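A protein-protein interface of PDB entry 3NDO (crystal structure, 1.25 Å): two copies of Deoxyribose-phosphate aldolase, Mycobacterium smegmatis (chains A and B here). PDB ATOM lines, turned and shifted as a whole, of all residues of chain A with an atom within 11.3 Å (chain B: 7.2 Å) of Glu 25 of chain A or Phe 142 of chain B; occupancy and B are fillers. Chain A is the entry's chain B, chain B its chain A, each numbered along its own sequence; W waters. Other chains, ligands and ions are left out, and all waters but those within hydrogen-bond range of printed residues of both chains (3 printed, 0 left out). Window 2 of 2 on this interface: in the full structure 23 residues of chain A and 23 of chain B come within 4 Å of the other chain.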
ATOM      1  N   LEU A  21      28.403   4.611   4.293  1.00  0.00           N
ATOM      2  CA  LEU A  21      28.111   5.997   3.890  1.00  0.00           C
ATOM      3  C   LEU A  21      27.190   5.931   2.682  1.00  0.00           C
ATOM      4  O   LEU A  21      27.583   5.384   1.667  1.00  0.00           O
ATOM      5  CB  LEU A  21      29.366   6.763   3.542  1.00  0.00           C
ATOM      6  CG  LEU A  21      29.108   8.215   3.012  1.00  0.00           C
ATOM      7  CD1 LEU A  21      28.390   9.114   4.041  1.00  0.00           C
ATOM      8  CD2 LEU A  21      30.438   8.770   2.510  1.00  0.00           C
ATOM      9  N   LEU A  22      26.015   6.505   2.816  1.00  0.00           N
ATOM     10  CA  LEU A  22      24.990   6.445   1.802  1.00  0.00           C
ATOM     11  C   LEU A  22      24.345   7.799   1.537  1.00  0.00           C
ATOM     12  O   LEU A  22      23.346   7.886   0.848  1.00  0.00           O
ATOM     13  CB  LEU A  22      23.959   5.378   2.146  1.00  0.00           C
ATOM     14  CG  LEU A  22      24.477   3.962   2.165  1.00  0.00           C
ATOM     15  CD1 LEU A  22      23.581   2.990   2.842  1.00  0.00           C
ATOM     16  CD2 LEU A  22      24.908   3.437   0.797  1.00  0.00           C
ATOM     17  N   LYS A  23      24.893   8.876   2.003  1.00  0.00           N
ATOM     18  CA  LYS A  23      24.306  10.197   1.764  1.00  0.00           C
ATOM     19  C   LYS A  23      24.278  10.519   0.275  1.00  0.00           C
ATOM     20  O   LYS A  23      25.265  10.313  -0.447  1.00  0.00           O
ATOM     21  CB  LYS A  23      25.079  11.262   2.529  1.00  0.00           C
ATOM     22  N   PRO A  24      23.222  11.169  -0.188  1.00  0.00           N
ATOM     23  CA  PRO A  24      23.207  11.620  -1.610  1.00  0.00           C
ATOM     24  C   PRO A  24      24.391  12.478  -1.995  1.00  0.00           C
ATOM     25  O   PRO A  24      24.781  12.462  -3.147  1.00  0.00           O
ATOM     26  CB  PRO A  24      21.880  12.336  -1.709  1.00  0.00           C
ATOM     27  CG  PRO A  24      20.988  11.642  -0.720  1.00  0.00           C
ATOM     28  CD  PRO A  24      21.912  11.380   0.469  1.00  0.00           C
ATOM     29  N   GLU A  25      24.865  13.305  -1.088  1.00  0.00           N
ATOM     30  CA  GLU A  25      25.936  14.231  -1.375  1.00  0.00           C
ATOM     31  C   GLU A  25      27.316  13.631  -1.245  1.00  0.00           C
ATOM     32  O   GLU A  25      28.277  14.330  -1.418  1.00  0.00           O
ATOM     33  CB  GLU A  25      25.797  15.484  -0.487  1.00  0.00           C
ATOM     34  CG  GLU A  25      25.949  15.248   0.956  1.00  0.00           C
ATOM     35  CD  GLU A  25      24.683  14.943   1.728  1.00  0.00           C
ATOM     36  OE1 GLU A  25      23.695  14.412   1.170  1.00  0.00           O
ATOM     37  OE2 GLU A  25      24.688  15.168   2.968  1.00  0.00           O
ATOM     38  N   ALA A  26      27.426  12.322  -1.027  1.00  0.00           N
ATOM     39  CA  ALA A  26      28.748  11.716  -0.857  1.00  0.00           C
ATOM     40  C   ALA A  26      29.588  11.836  -2.116  1.00  0.00           C
ATOM     41  O   ALA A  26      29.110  11.633  -3.238  1.00  0.00           O
ATOM     42  CB  ALA A  26      28.622  10.246  -0.517  1.00  0.00           C
ATOM     43  N   THR A  27      30.846  12.165  -1.933  1.00  0.00           N
ATOM     44  CA  THR A  27      31.788  12.318  -3.003  1.00  0.00           C
ATOM     45  C   THR A  27      32.804  11.159  -3.008  1.00  0.00           C
ATOM     46  O   THR A  27      32.926  10.426  -2.018  1.00  0.00           O
ATOM     47  CB  THR A  27      32.583  13.611  -2.824  1.00  0.00           C
ATOM     48  OG1 THR A  27      33.327  13.468  -1.626  1.00  0.00           O
ATOM     49  CG2 THR A  27      31.669  14.844  -2.785  1.00  0.00           C
ATOM     50  N   PRO A  28      33.610  11.021  -4.063  1.00  0.00           N
ATOM     51  CA  PRO A  28      34.702  10.019  -4.037  1.00  0.00           C
ATOM     52  C   PRO A  28      35.647  10.173  -2.866  1.00  0.00           C
ATOM     53  O   PRO A  28      36.026   9.187  -2.255  1.00  0.00           O
ATOM     54  CB  PRO A  28      35.381  10.209  -5.397  1.00  0.00           C
ATOM     55  CG  PRO A  28      34.206  10.644  -6.274  1.00  0.00           C
ATOM     56  CD  PRO A  28      33.429  11.596  -5.406  1.00  0.00           C
ATOM     57  N   SER A  29      35.969  11.423  -2.501  1.00  0.00           N
ATOM     58  CA  SER A  29      36.849  11.671  -1.353  1.00  0.00           C
ATOM     59  C   SER A  29      36.227  11.202  -0.066  1.00  0.00           C
ATOM     60  O   SER A  29      36.889  10.672   0.834  1.00  0.00           O
ATOM     61  CB  SER A  29      37.098  13.186  -1.328  1.00  0.00           C
ATOM     62  OG  SER A  29      38.010  13.506  -2.378  1.00  0.00           O
ATOM     63  N   ASP A  30      34.919  11.358   0.045  1.00  0.00           N
ATOM     64  CA  ASP A  30      34.239  10.850   1.238  1.00  0.00           C
ATOM     65  C   ASP A  30      34.340   9.337   1.320  1.00  0.00           C
ATOM     66  O   ASP A  30      34.463   8.764   2.417  1.00  0.00           O
ATOM     67  CB  ASP A  30      32.740  11.226   1.226  1.00  0.00           C
ATOM     68  CG  ASP A  30      32.467  12.724   1.327  1.00  0.00           C
ATOM     69  OD1 ASP A  30      33.279  13.480   1.889  1.00  0.00           O
ATOM     70  OD2 ASP A  30      31.360  13.165   0.923  1.00  0.00           O
ATOM     71  N   VAL A  31      34.275   8.651   0.191  1.00  0.00           N
ATOM     72  CA  VAL A  31      34.339   7.201   0.147  1.00  0.00           C
ATOM     73  C   VAL A  31      35.751   6.714   0.428  1.00  0.00           C
ATOM     74  O   VAL A  31      35.937   5.732   1.136  1.00  0.00           O
ATOM     75  CB  VAL A  31      33.691   6.637  -1.091  1.00  0.00           C
ATOM     76  CG1 VAL A  31      34.008   5.162  -1.292  1.00  0.00           C
ATOM     77  CG2 VAL A  31      32.170   6.859  -1.022  1.00  0.00           C
ATOM     78  N   THR A  32      36.783   7.391  -0.098  1.00  0.00           N
ATOM     79  CA  THR A  32      38.134   6.948   0.251  1.00  0.00           C
ATOM     80  C   THR A  32      38.401   7.169   1.736  1.00  0.00           C
ATOM     81  O   THR A  32      39.043   6.315   2.405  1.00  0.00           O
ATOM     82  CB  THR A  32      39.172   7.568  -0.660  1.00  0.00           C
ATOM     83  OG1 THR A  32      39.182   8.967  -0.462  1.00  0.00           O
ATOM     84  CG2 THR A  32      38.886   7.207  -2.089  1.00  0.00           C
ATOM     85  N   VAL A  48      28.448   1.179   0.440  1.00  0.00           N
ATOM     86  CA  VAL A  48      28.376   2.406  -0.330  1.00  0.00           C
ATOM     87  C   VAL A  48      27.295   2.338  -1.384  1.00  0.00           C
ATOM     88  O   VAL A  48      26.726   1.264  -1.678  1.00  0.00           O
ATOM     89  CB  VAL A  48      29.769   2.775  -0.986  1.00  0.00           C
ATOM     90  CG1 VAL A  48      30.861   2.920   0.073  1.00  0.00           C
ATOM     91  CG2 VAL A  48      30.168   1.739  -2.023  1.00  0.00           C
ATOM     92  N   SER A  49      27.014   3.482  -1.995  1.00  0.00           N
ATOM     93  CA  SER A  49      26.055   3.550  -3.036  1.00  0.00           C
ATOM     94  C   SER A  49      26.605   3.028  -4.362  1.00  0.00           C
ATOM     95  O   SER A  49      27.807   3.076  -4.629  1.00  0.00           O
ATOM     96  CB  SER A  49      25.633   5.033  -3.223  1.00  0.00           C
ATOM     97  OG  SER A  49      25.043   5.609  -2.075  1.00  0.00           O
ATOM     98  N   PRO A  51      27.120   4.092  -7.513  1.00  0.00           N
ATOM     99  CA  PRO A  51      28.073   4.776  -8.339  1.00  0.00           C
ATOM    100  C   PRO A  51      29.419   4.929  -7.678  1.00  0.00           C
ATOM    101  O   PRO A  51      30.339   5.399  -8.333  1.00  0.00           O
ATOM    102  CB  PRO A  51      27.430   6.118  -8.562  1.00  0.00           C
ATOM    103  CG  PRO A  51      26.057   6.021  -8.186  1.00  0.00           C
ATOM    104  CD  PRO A  51      25.985   4.980  -7.165  1.00  0.00           C
ATOM    105  N   LEU A  52      29.545   4.594  -6.390  1.00  0.00           N
ATOM    106  CA  LEU A  52      30.772   4.782  -5.648  1.00  0.00           C
ATOM    107  C   LEU A  52      31.467   3.465  -5.338  1.00  0.00           C
ATOM    108  O   LEU A  52      32.557   3.435  -4.760  1.00  0.00           O
ATOM    109  CB  LEU A  52      30.509   5.587  -4.373  1.00  0.00           C
ATOM    110  CG  LEU A  52      30.292   7.088  -4.647  1.00  0.00           C
ATOM    111  CD1 LEU A  52      29.565   7.779  -3.515  1.00  0.00           C
ATOM    112  CD2 LEU A  52      31.605   7.762  -4.860  1.00  0.00           C
ATOM    113  N   PHE A  72      17.697   1.512  -3.519  1.00  0.00           N
ATOM    114  CA  PHE A  72      17.812   2.144  -2.196  1.00  0.00           C
ATOM    115  C   PHE A  72      17.738   3.649  -2.280  1.00  0.00           C
ATOM    116  O   PHE A  72      18.330   4.258  -3.168  1.00  0.00           O
ATOM    117  CB  PHE A  72      19.164   1.697  -1.603  1.00  0.00           C
ATOM    118  CG  PHE A  72      19.448   2.187  -0.221  1.00  0.00           C
ATOM    119  CD1 PHE A  72      19.342   1.323   0.863  1.00  0.00           C
ATOM    120  CD2 PHE A  72      19.905   3.491   0.022  1.00  0.00           C
ATOM    121  CE1 PHE A  72      19.601   1.782   2.146  1.00  0.00           C
ATOM    122  CE2 PHE A  72      20.184   3.930   1.302  1.00  0.00           C
ATOM    123  CZ  PHE A  72      20.021   3.064   2.362  1.00  0.00           C
ATOM    124  N   PRO A  73      17.087   4.337  -1.314  1.00  0.00           N
ATOM    125  CA  PRO A  73      16.435   3.796  -0.121  1.00  0.00           C
ATOM    126  C   PRO A  73      14.993   3.443  -0.265  1.00  0.00           C
ATOM    127  O   PRO A  73      14.413   2.879   0.669  1.00  0.00           O
ATOM    128  CB  PRO A  73      16.602   4.911   0.895  1.00  0.00           C
ATOM    129  CG  PRO A  73      16.467   6.133   0.031  1.00  0.00           C
ATOM    130  CD  PRO A  73      17.214   5.820  -1.214  1.00  0.00           C
ATOM    131  N   PHE A 169      16.573   5.603   6.387  1.00  0.00           N
ATOM    132  CA  PHE A 169      15.967   6.783   5.742  1.00  0.00           C
ATOM    133  C   PHE A 169      14.477   6.840   5.883  1.00  0.00           C
ATOM    134  O   PHE A 169      13.842   7.781   5.417  1.00  0.00           O
ATOM    135  CB  PHE A 169      16.341   6.802   4.258  1.00  0.00           C
ATOM    136  CG  PHE A 169      17.784   7.172   3.999  1.00  0.00           C
ATOM    137  CD1 PHE A 169      18.159   8.464   3.738  1.00  0.00           C
ATOM    138  CD2 PHE A 169      18.775   6.219   3.993  1.00  0.00           C
ATOM    139  CE1 PHE A 169      19.509   8.798   3.524  1.00  0.00           C
ATOM    140  CE2 PHE A 169      20.088   6.555   3.776  1.00  0.00           C
ATOM    141  CZ  PHE A 169      20.434   7.819   3.555  1.00  0.00           C
ATOM    142  N   SER B  74      17.600   9.413  -4.129  1.00  0.00           N
ATOM    143  CA  SER B  74      18.985   9.660  -3.789  1.00  0.00           C
ATOM    144  C   SER B  74      19.824  10.223  -4.884  1.00  0.00           C
ATOM    145  O   SER B  74      20.847  10.853  -4.581  1.00  0.00           O
ATOM    146  CB  SER B  74      19.660   8.436  -3.228  1.00  0.00           C
ATOM    147  OG  SER B  74      19.949   7.507  -4.310  1.00  0.00           O
ATOM    148  N   LYS B  76      21.676   8.402  -6.476  1.00  0.00           N
ATOM    149  CA  LYS B  76      22.903   7.547  -6.438  1.00  0.00           C
ATOM    150  C   LYS B  76      22.636   6.246  -7.192  1.00  0.00           C
ATOM    151  O   LYS B  76      22.503   5.168  -6.607  1.00  0.00           O
ATOM    152  CB  LYS B  76      23.355   7.301  -5.009  1.00  0.00           C
ATOM    153  CG  LYS B  76      24.033   8.482  -4.360  1.00  0.00           C
ATOM    154  CD  LYS B  76      25.339   8.847  -5.074  1.00  0.00           C
ATOM    155  CE  LYS B  76      26.211   9.693  -4.160  1.00  0.00           C
ATOM    156  NZ  LYS B  76      27.215  10.388  -4.903  1.00  0.00           N
ATOM    157  N   ASP B 102      23.131  13.112  -9.524  1.00  0.00           N
ATOM    158  CA  ASP B 102      24.077  12.716  -8.520  1.00  0.00           C
ATOM    159  C   ASP B 102      24.646  13.970  -7.868  1.00  0.00           C
ATOM    160  O   ASP B 102      25.515  14.658  -8.398  1.00  0.00           O
ATOM    161  CB  ASP B 102      25.139  11.806  -9.147  1.00  0.00           C
ATOM    162  CG  ASP B 102      26.121  11.236  -8.117  1.00  0.00           C
ATOM    163  OD1 ASP B 102      26.295  11.847  -7.035  1.00  0.00           O
ATOM    164  OD2 ASP B 102      26.715  10.173  -8.426  1.00  0.00           O
ATOM    165  N   VAL B 103      24.078  14.295  -6.726  1.00  0.00           N
ATOM    166  CA  VAL B 103      24.408  15.486  -5.979  1.00  0.00           C
ATOM    167  C   VAL B 103      25.878  15.519  -5.576  1.00  0.00           C
ATOM    168  O   VAL B 103      26.563  16.549  -5.630  1.00  0.00           O
ATOM    169  CB  VAL B 103      23.478  15.628  -4.772  1.00  0.00           C
ATOM    170  CG1 VAL B 103      23.868  16.809  -3.918  1.00  0.00           C
ATOM    171  CG2 VAL B 103      21.993  15.600  -5.213  1.00  0.00           C
ATOM    172  N   GLY B 104      26.403  14.381  -5.169  1.00  0.00           N
ATOM    173  CA  GLY B 104      27.793  14.253  -4.782  1.00  0.00           C
ATOM    174  C   GLY B 104      28.705  14.500  -5.947  1.00  0.00           C
ATOM    175  O   GLY B 104      29.776  15.141  -5.775  1.00  0.00           O
ATOM    176  N   ALA B 105      28.371  14.034  -7.149  1.00  0.00           N
ATOM    177  CA  ALA B 105      29.147  14.366  -8.343  1.00  0.00           C
ATOM    178  C   ALA B 105      29.207  15.877  -8.540  1.00  0.00           C
ATOM    179  O   ALA B 105      30.283  16.427  -8.848  1.00  0.00           O
ATOM    180  CB  ALA B 105      28.621  13.666  -9.606  1.00  0.00           C
ATOM    181  N   LEU B 107      28.892  18.215  -6.262  1.00  0.00           N
ATOM    182  CA  LEU B 107      29.673  18.803  -5.200  1.00  0.00           C
ATOM    183  C   LEU B 107      31.157  18.521  -5.332  1.00  0.00           C
ATOM    184  O   LEU B 107      31.970  19.323  -4.881  1.00  0.00           O
ATOM    185  CB  LEU B 107      29.175  18.337  -3.831  1.00  0.00           C
ATOM    186  CG  LEU B 107      27.824  18.948  -3.464  1.00  0.00           C
ATOM    187  CD1 LEU B 107      27.211  18.266  -2.268  1.00  0.00           C
ATOM    188  CD2 LEU B 107      27.967  20.404  -3.210  1.00  0.00           C
ATOM    189  N   ALA B 108      31.511  17.419  -5.959  1.00  0.00           N
ATOM    190  CA  ALA B 108      32.904  17.076  -6.260  1.00  0.00           C
ATOM    191  C   ALA B 108      33.426  17.876  -7.438  1.00  0.00           C
ATOM    192  O   ALA B 108      34.629  17.823  -7.704  1.00  0.00           O
ATOM    193  CB  ALA B 108      33.014  15.628  -6.563  1.00  0.00           C
ATOM    194  N   SER B 136      18.400  21.648  -4.929  1.00  0.00           N
ATOM    195  CA  SER B 136      18.922  22.970  -4.763  1.00  0.00           C
ATOM    196  C   SER B 136      19.277  23.307  -3.334  1.00  0.00           C
ATOM    197  O   SER B 136      20.259  24.017  -3.122  1.00  0.00           O
ATOM    198  CB  SER B 136      17.937  23.984  -5.301  1.00  0.00           C
ATOM    199  OG  SER B 136      16.638  23.867  -4.742  1.00  0.00           O
ATOM    200  N   ALA B 137      18.520  22.814  -2.353  1.00  0.00           N
ATOM    201  CA  ALA B 137      18.857  23.138  -0.966  1.00  0.00           C
ATOM    202  C   ALA B 137      20.209  22.567  -0.602  1.00  0.00           C
ATOM    203  O   ALA B 137      20.964  23.186   0.176  1.00  0.00           O
ATOM    204  CB  ALA B 137      17.805  22.670  -0.012  1.00  0.00           C
ATOM    205  N   ALA B 138      20.549  21.385  -1.118  1.00  0.00           N
ATOM    206  CA  ALA B 138      21.842  20.766  -0.841  1.00  0.00           C
ATOM    207  C   ALA B 138      22.958  21.502  -1.590  1.00  0.00           C
ATOM    208  O   ALA B 138      24.024  21.754  -1.032  1.00  0.00           O
ATOM    209  CB  ALA B 138      21.829  19.289  -1.223  1.00  0.00           C
ATOM    210  N   LEU B 139      22.739  21.844  -2.840  1.00  0.00           N
ATOM    211  CA  LEU B 139      23.768  22.586  -3.588  1.00  0.00           C
ATOM    212  C   LEU B 139      24.063  23.921  -2.901  1.00  0.00           C
ATOM    213  O   LEU B 139      25.234  24.307  -2.834  1.00  0.00           O
ATOM    214  CB  LEU B 139      23.351  22.814  -5.034  1.00  0.00           C
ATOM    215  CG  LEU B 139      23.115  21.550  -5.896  1.00  0.00           C
ATOM    216  CD1 LEU B 139      22.707  21.976  -7.302  1.00  0.00           C
ATOM    217  CD2 LEU B 139      24.258  20.609  -5.882  1.00  0.00           C
ATOM    218  N   LEU B 140      23.036  24.614  -2.432  1.00  0.00           N
ATOM    219  CA  LEU B 140      23.224  25.862  -1.747  1.00  0.00           C
ATOM    220  C   LEU B 140      23.903  25.680  -0.416  1.00  0.00           C
ATOM    221  O   LEU B 140      24.797  26.454  -0.065  1.00  0.00           O
ATOM    222  CB  LEU B 140      21.900  26.606  -1.598  1.00  0.00           C
ATOM    223  CG  LEU B 140      21.314  27.156  -2.887  1.00  0.00           C
ATOM    224  CD1 LEU B 140      19.893  27.637  -2.653  1.00  0.00           C
ATOM    225  CD2 LEU B 140      22.180  28.281  -3.433  1.00  0.00           C
ATOM    226  N   GLU B 141      23.529  24.685   0.354  1.00  0.00           N
ATOM    227  CA  GLU B 141      24.097  24.460   1.703  1.00  0.00           C
ATOM    228  C   GLU B 141      25.554  24.100   1.600  1.00  0.00           C
ATOM    229  O   GLU B 141      26.388  24.581   2.411  1.00  0.00           O
ATOM    230  CB  GLU B 141      23.330  23.362   2.423  1.00  0.00           C
ATOM    231  CG  GLU B 141      23.926  23.017   3.790  1.00  0.00           C
ATOM    232  CD  GLU B 141      23.159  22.022   4.590  1.00  0.00           C
ATOM    233  OE1 GLU B 141      22.019  21.683   4.275  1.00  0.00           O
ATOM    234  OE2 GLU B 141      23.703  21.569   5.636  1.00  0.00           O
ATOM    235  N   PHE B 142      25.909  23.204   0.690  1.00  0.00           N
ATOM    236  CA  PHE B 142      27.237  22.608   0.693  1.00  0.00           C
ATOM    237  C   PHE B 142      28.200  23.335  -0.241  1.00  0.00           C
ATOM    238  O   PHE B 142      29.399  23.070  -0.193  1.00  0.00           O
ATOM    239  CB  PHE B 142      27.164  21.130   0.365  1.00  0.00           C
ATOM    240  CG  PHE B 142      26.475  20.323   1.416  1.00  0.00           C
ATOM    241  CD1 PHE B 142      27.078  20.218   2.679  1.00  0.00           C
ATOM    242  CD2 PHE B 142      25.354  19.648   1.183  1.00  0.00           C
ATOM    243  CE1 PHE B 142      26.474  19.510   3.687  1.00  0.00           C
ATOM    244  CE2 PHE B 142      24.702  18.955   2.210  1.00  0.00           C
ATOM    245  CZ  PHE B 142      25.293  18.926   3.444  1.00  0.00           C
ATOM    246  N   SER B 143      27.721  24.182  -1.120  1.00  0.00           N
ATOM    247  CA  SER B 143      28.561  24.921  -2.043  1.00  0.00           C
ATOM    248  C   SER B 143      28.167  26.366  -2.163  1.00  0.00           C
ATOM    249  O   SER B 143      28.889  27.272  -1.724  1.00  0.00           O
ATOM    250  CB  SER B 143      28.619  24.223  -3.388  1.00  0.00           C
ATOM    251  OG  SER B 143      29.453  24.933  -4.281  1.00  0.00           O
ATOM    252  N   GLY B 144      27.056  26.637  -2.810  1.00  0.00           N
ATOM    253  CA  GLY B 144      26.539  28.006  -2.949  1.00  0.00           C
ATOM    254  C   GLY B 144      25.847  28.228  -4.276  1.00  0.00           C
ATOM    255  O   GLY B 144      25.559  27.308  -5.029  1.00  0.00           O
ATOM    256  N   LEU B 147      27.265  27.072  -7.942  1.00  0.00           N
ATOM    257  CA  LEU B 147      27.094  25.677  -8.274  1.00  0.00           C
ATOM    258  C   LEU B 147      25.659  25.402  -8.725  1.00  0.00           C
ATOM    259  O   LEU B 147      25.424  24.655  -9.695  1.00  0.00           O
ATOM    260  CB  LEU B 147      27.500  24.716  -7.170  1.00  0.00           C
ATOM    261  CG  LEU B 147      27.329  23.239  -7.517  1.00  0.00           C
ATOM    262  CD1 LEU B 147      28.178  22.786  -8.704  1.00  0.00           C
ATOM    263  CD2 LEU B 147      27.674  22.388  -6.274  1.00  0.00           C
ATOM    264  N   HIS B 170      15.486  15.236   1.101  1.00  0.00           N
ATOM    265  CA  HIS B 170      16.850  15.546   1.533  1.00  0.00           C
ATOM    266  C   HIS B 170      16.809  16.440   2.762  1.00  0.00           C
ATOM    267  O   HIS B 170      16.055  17.411   2.801  1.00  0.00           O
ATOM    268  CB  HIS B 170      17.640  16.244   0.411  1.00  0.00           C
ATOM    269  CG  HIS B 170      19.089  16.269   0.674  1.00  0.00           C
ATOM    270  ND1 HIS B 170      19.684  17.130   1.562  1.00  0.00           N
ATOM    271  CD2 HIS B 170      20.047  15.452   0.206  1.00  0.00           C
ATOM    272  CE1 HIS B 170      20.971  16.804   1.644  1.00  0.00           C
ATOM    273  NE2 HIS B 170      21.216  15.769   0.859  1.00  0.00           N
ATOM    274  N   PRO B 171      17.644  16.173   3.784  1.00  0.00           N
ATOM    275  CA  PRO B 171      17.617  16.988   5.019  1.00  0.00           C
ATOM    276  C   PRO B 171      17.974  18.453   4.819  1.00  0.00           C
ATOM    277  O   PRO B 171      17.623  19.270   5.689  1.00  0.00           O
ATOM    278  CB  PRO B 171      18.634  16.283   5.928  1.00  0.00           C
ATOM    279  CG  PRO B 171      19.054  15.139   5.296  1.00  0.00           C
ATOM    280  CD  PRO B 171      18.543  15.020   3.910  1.00  0.00           C
ATOM    281  N   SER B 172      18.602  18.840   3.716  1.00  0.00           N
ATOM    282  CA  SER B 172      18.923  20.241   3.466  1.00  0.00           C
ATOM    283  C   SER B 172      17.641  21.050   3.230  1.00  0.00           C
ATOM    284  O   SER B 172      17.667  22.250   3.384  1.00  0.00           O
ATOM    285  CB  SER B 172      19.873  20.419   2.287  1.00  0.00           C
ATOM    286  OG  SER B 172      21.148  19.817   2.517  1.00  0.00           O
HETATM  287  O   HOH W   1      17.407   6.530  -4.733  1.00  0.00           O
HETATM  288  O   HOH W   2      23.148  11.935  -5.408  1.00  0.00           O
HETATM  289  O   HOH W   3      21.070   4.324  -4.356  1.00  0.00           O
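The side-chain amino group (NZ) of Lys 76 of chain B lies within hydrogen-bond range of the backbone carbonyl oxygen (O) of Ala 26 of chain A (2.8 Å).
O of Pro 24 of chain A lies within hydrogen-bond range of N of Gly 104 of chain B.
The side-chain carboxylate (OE1) of Glu 25 of chain A sits at hydrogen-bond distance from a ring nitrogen (NE2) of His 170 of chain B (2.8 Å).
N of Lys 76 of chain B is in hydrogen-bond range of OG of Ser 74 of chain B (2.9 Å).
NZ of Lys 76 of chain B is in salt-bridge range of OD1 of Asp 102 of chain B, at 2.7 Å.
The side-chain carboxylate (OD1) of Asp 102 of chain B sits at hydrogen-bond distance from the backbone NH (N) of Gly 104 of chain B (3.1 Å).
A ring nitrogen (ND1) of His 170 of chain B lies within hydrogen-bond range of the backbone NH of Ser 172 of chain B, 3.0 Å away.
The side-chain hydroxyl of Thr 27 of chain A lies close to the backbone NH of Ser 29 of chain A.
The side-chain carboxylate of Asp 30 of chain A lies within hydrogen-bond range of the backbone NH of Thr 27 of chain A (3.1 Å).
Lys 23 of chain A touches Lys 76 of chain B (O to CE, 3.9 Å).
Ser 74 of chain B touches Pro 24 of chain A.
O of Pro 24 of chain A touches CE of Lys 76 of chain B (3.3 Å).
Glu 25 of chain A touches Gly 104 of chain B.
CB of Glu 25 of chain A touches CD1 of Leu 107 of chain B, 3.6 Å away.
Glu 25 of chain A touches Phe 142 of chain B.
Gly 104 of chain B touches Thr 27 of chain A.
Lys 76 of chain B touches Ser 49 of chain A (CB to CB, 3.7 Å).
NZ of Lys 76 of chain B touches CD1 of Leu 52 of chain A (3.8 Å).
OG of Ser 74 of chain B touches O of Phe 72 of chain A, at 3.8 Å.
Of chain B, only Gly 104 (3.4 Å), Leu 107 (3.6 Å), Phe 142 (3.8 Å) and His 170 (2.8 Å) come within 4 Å of Glu 25 of chain A.
Of chain A, only Glu 25 comes within 4 Å of Phe 142 of chain B.
Of chain A, only Pro 24 (3.8 Å) comes within 4 Å of Val 103 of chain B.
Of chain A, only Pro 24 (3.2 Å), Glu 25 (3.4 Å), Ala 26 (3.3 Å) and Thr 27 (3.6 Å) come within 4 Å of Gly 104 of chain B.
Leu 107 of chain B touches just one residue of chain A: Glu 25.
No residue of chain A comes within 4 Å of Glu 141 of chain B.
No residue of chain A comes within 4 Å of Ser 143 of chain B.
No residue of chain A comes within 4 Å of Gly 144 of chain B.
Printed residues of chain B within 4 Å of Ser 49 of chain A: Lys 76.
Printed residues of chain B within 4 Å of Leu 52 of chain A: Lys 76.
Printed residues of chain B within 4 Å of Phe 72 of chain A: Ser 74 (3.8 Å).
Of the printed residues of chain B, Pro 24 of chain A touches Ser 74, Lys 76, Val 103 and Gly 104.
The nearest residue of chain B that does not touch Glu 25 of chain A is Val 103 of chain B (4.2 Å).
The nearest printed residue of chain B that does not touch Thr 27 of chain A is Ala 108 of chain B (4.1 Å).
Hydrophobic or aromatic side chains of chain A that line the printed part of chain B: Pro 24, Pro 51 and Leu 52.
Of the 21 printed residues of chain B, 7 touch a printed residue of chain A.
No position is printed for both chains.
Water W2 lies within hydrogen-bond range of O of Ser 74 of chain B (2.7 Å), O of Pro 24 of chain A (2.8 Å) and N of Val 103 of chain B (2.9 Å).
Water W1 lies within hydrogen-bond range of OG of Ser 74 of chain B and O of Phe 72 of chain A.
Water W3 lies within hydrogen-bond range of the backbone carbonyl oxygen of Lys 76 of chain B (2.8 Å), the backbone carbonyl oxygen of Phe 72 of chain A (3.0 Å) and the side-chain hydroxyl of Ser 74 of chain B (3.4 Å).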
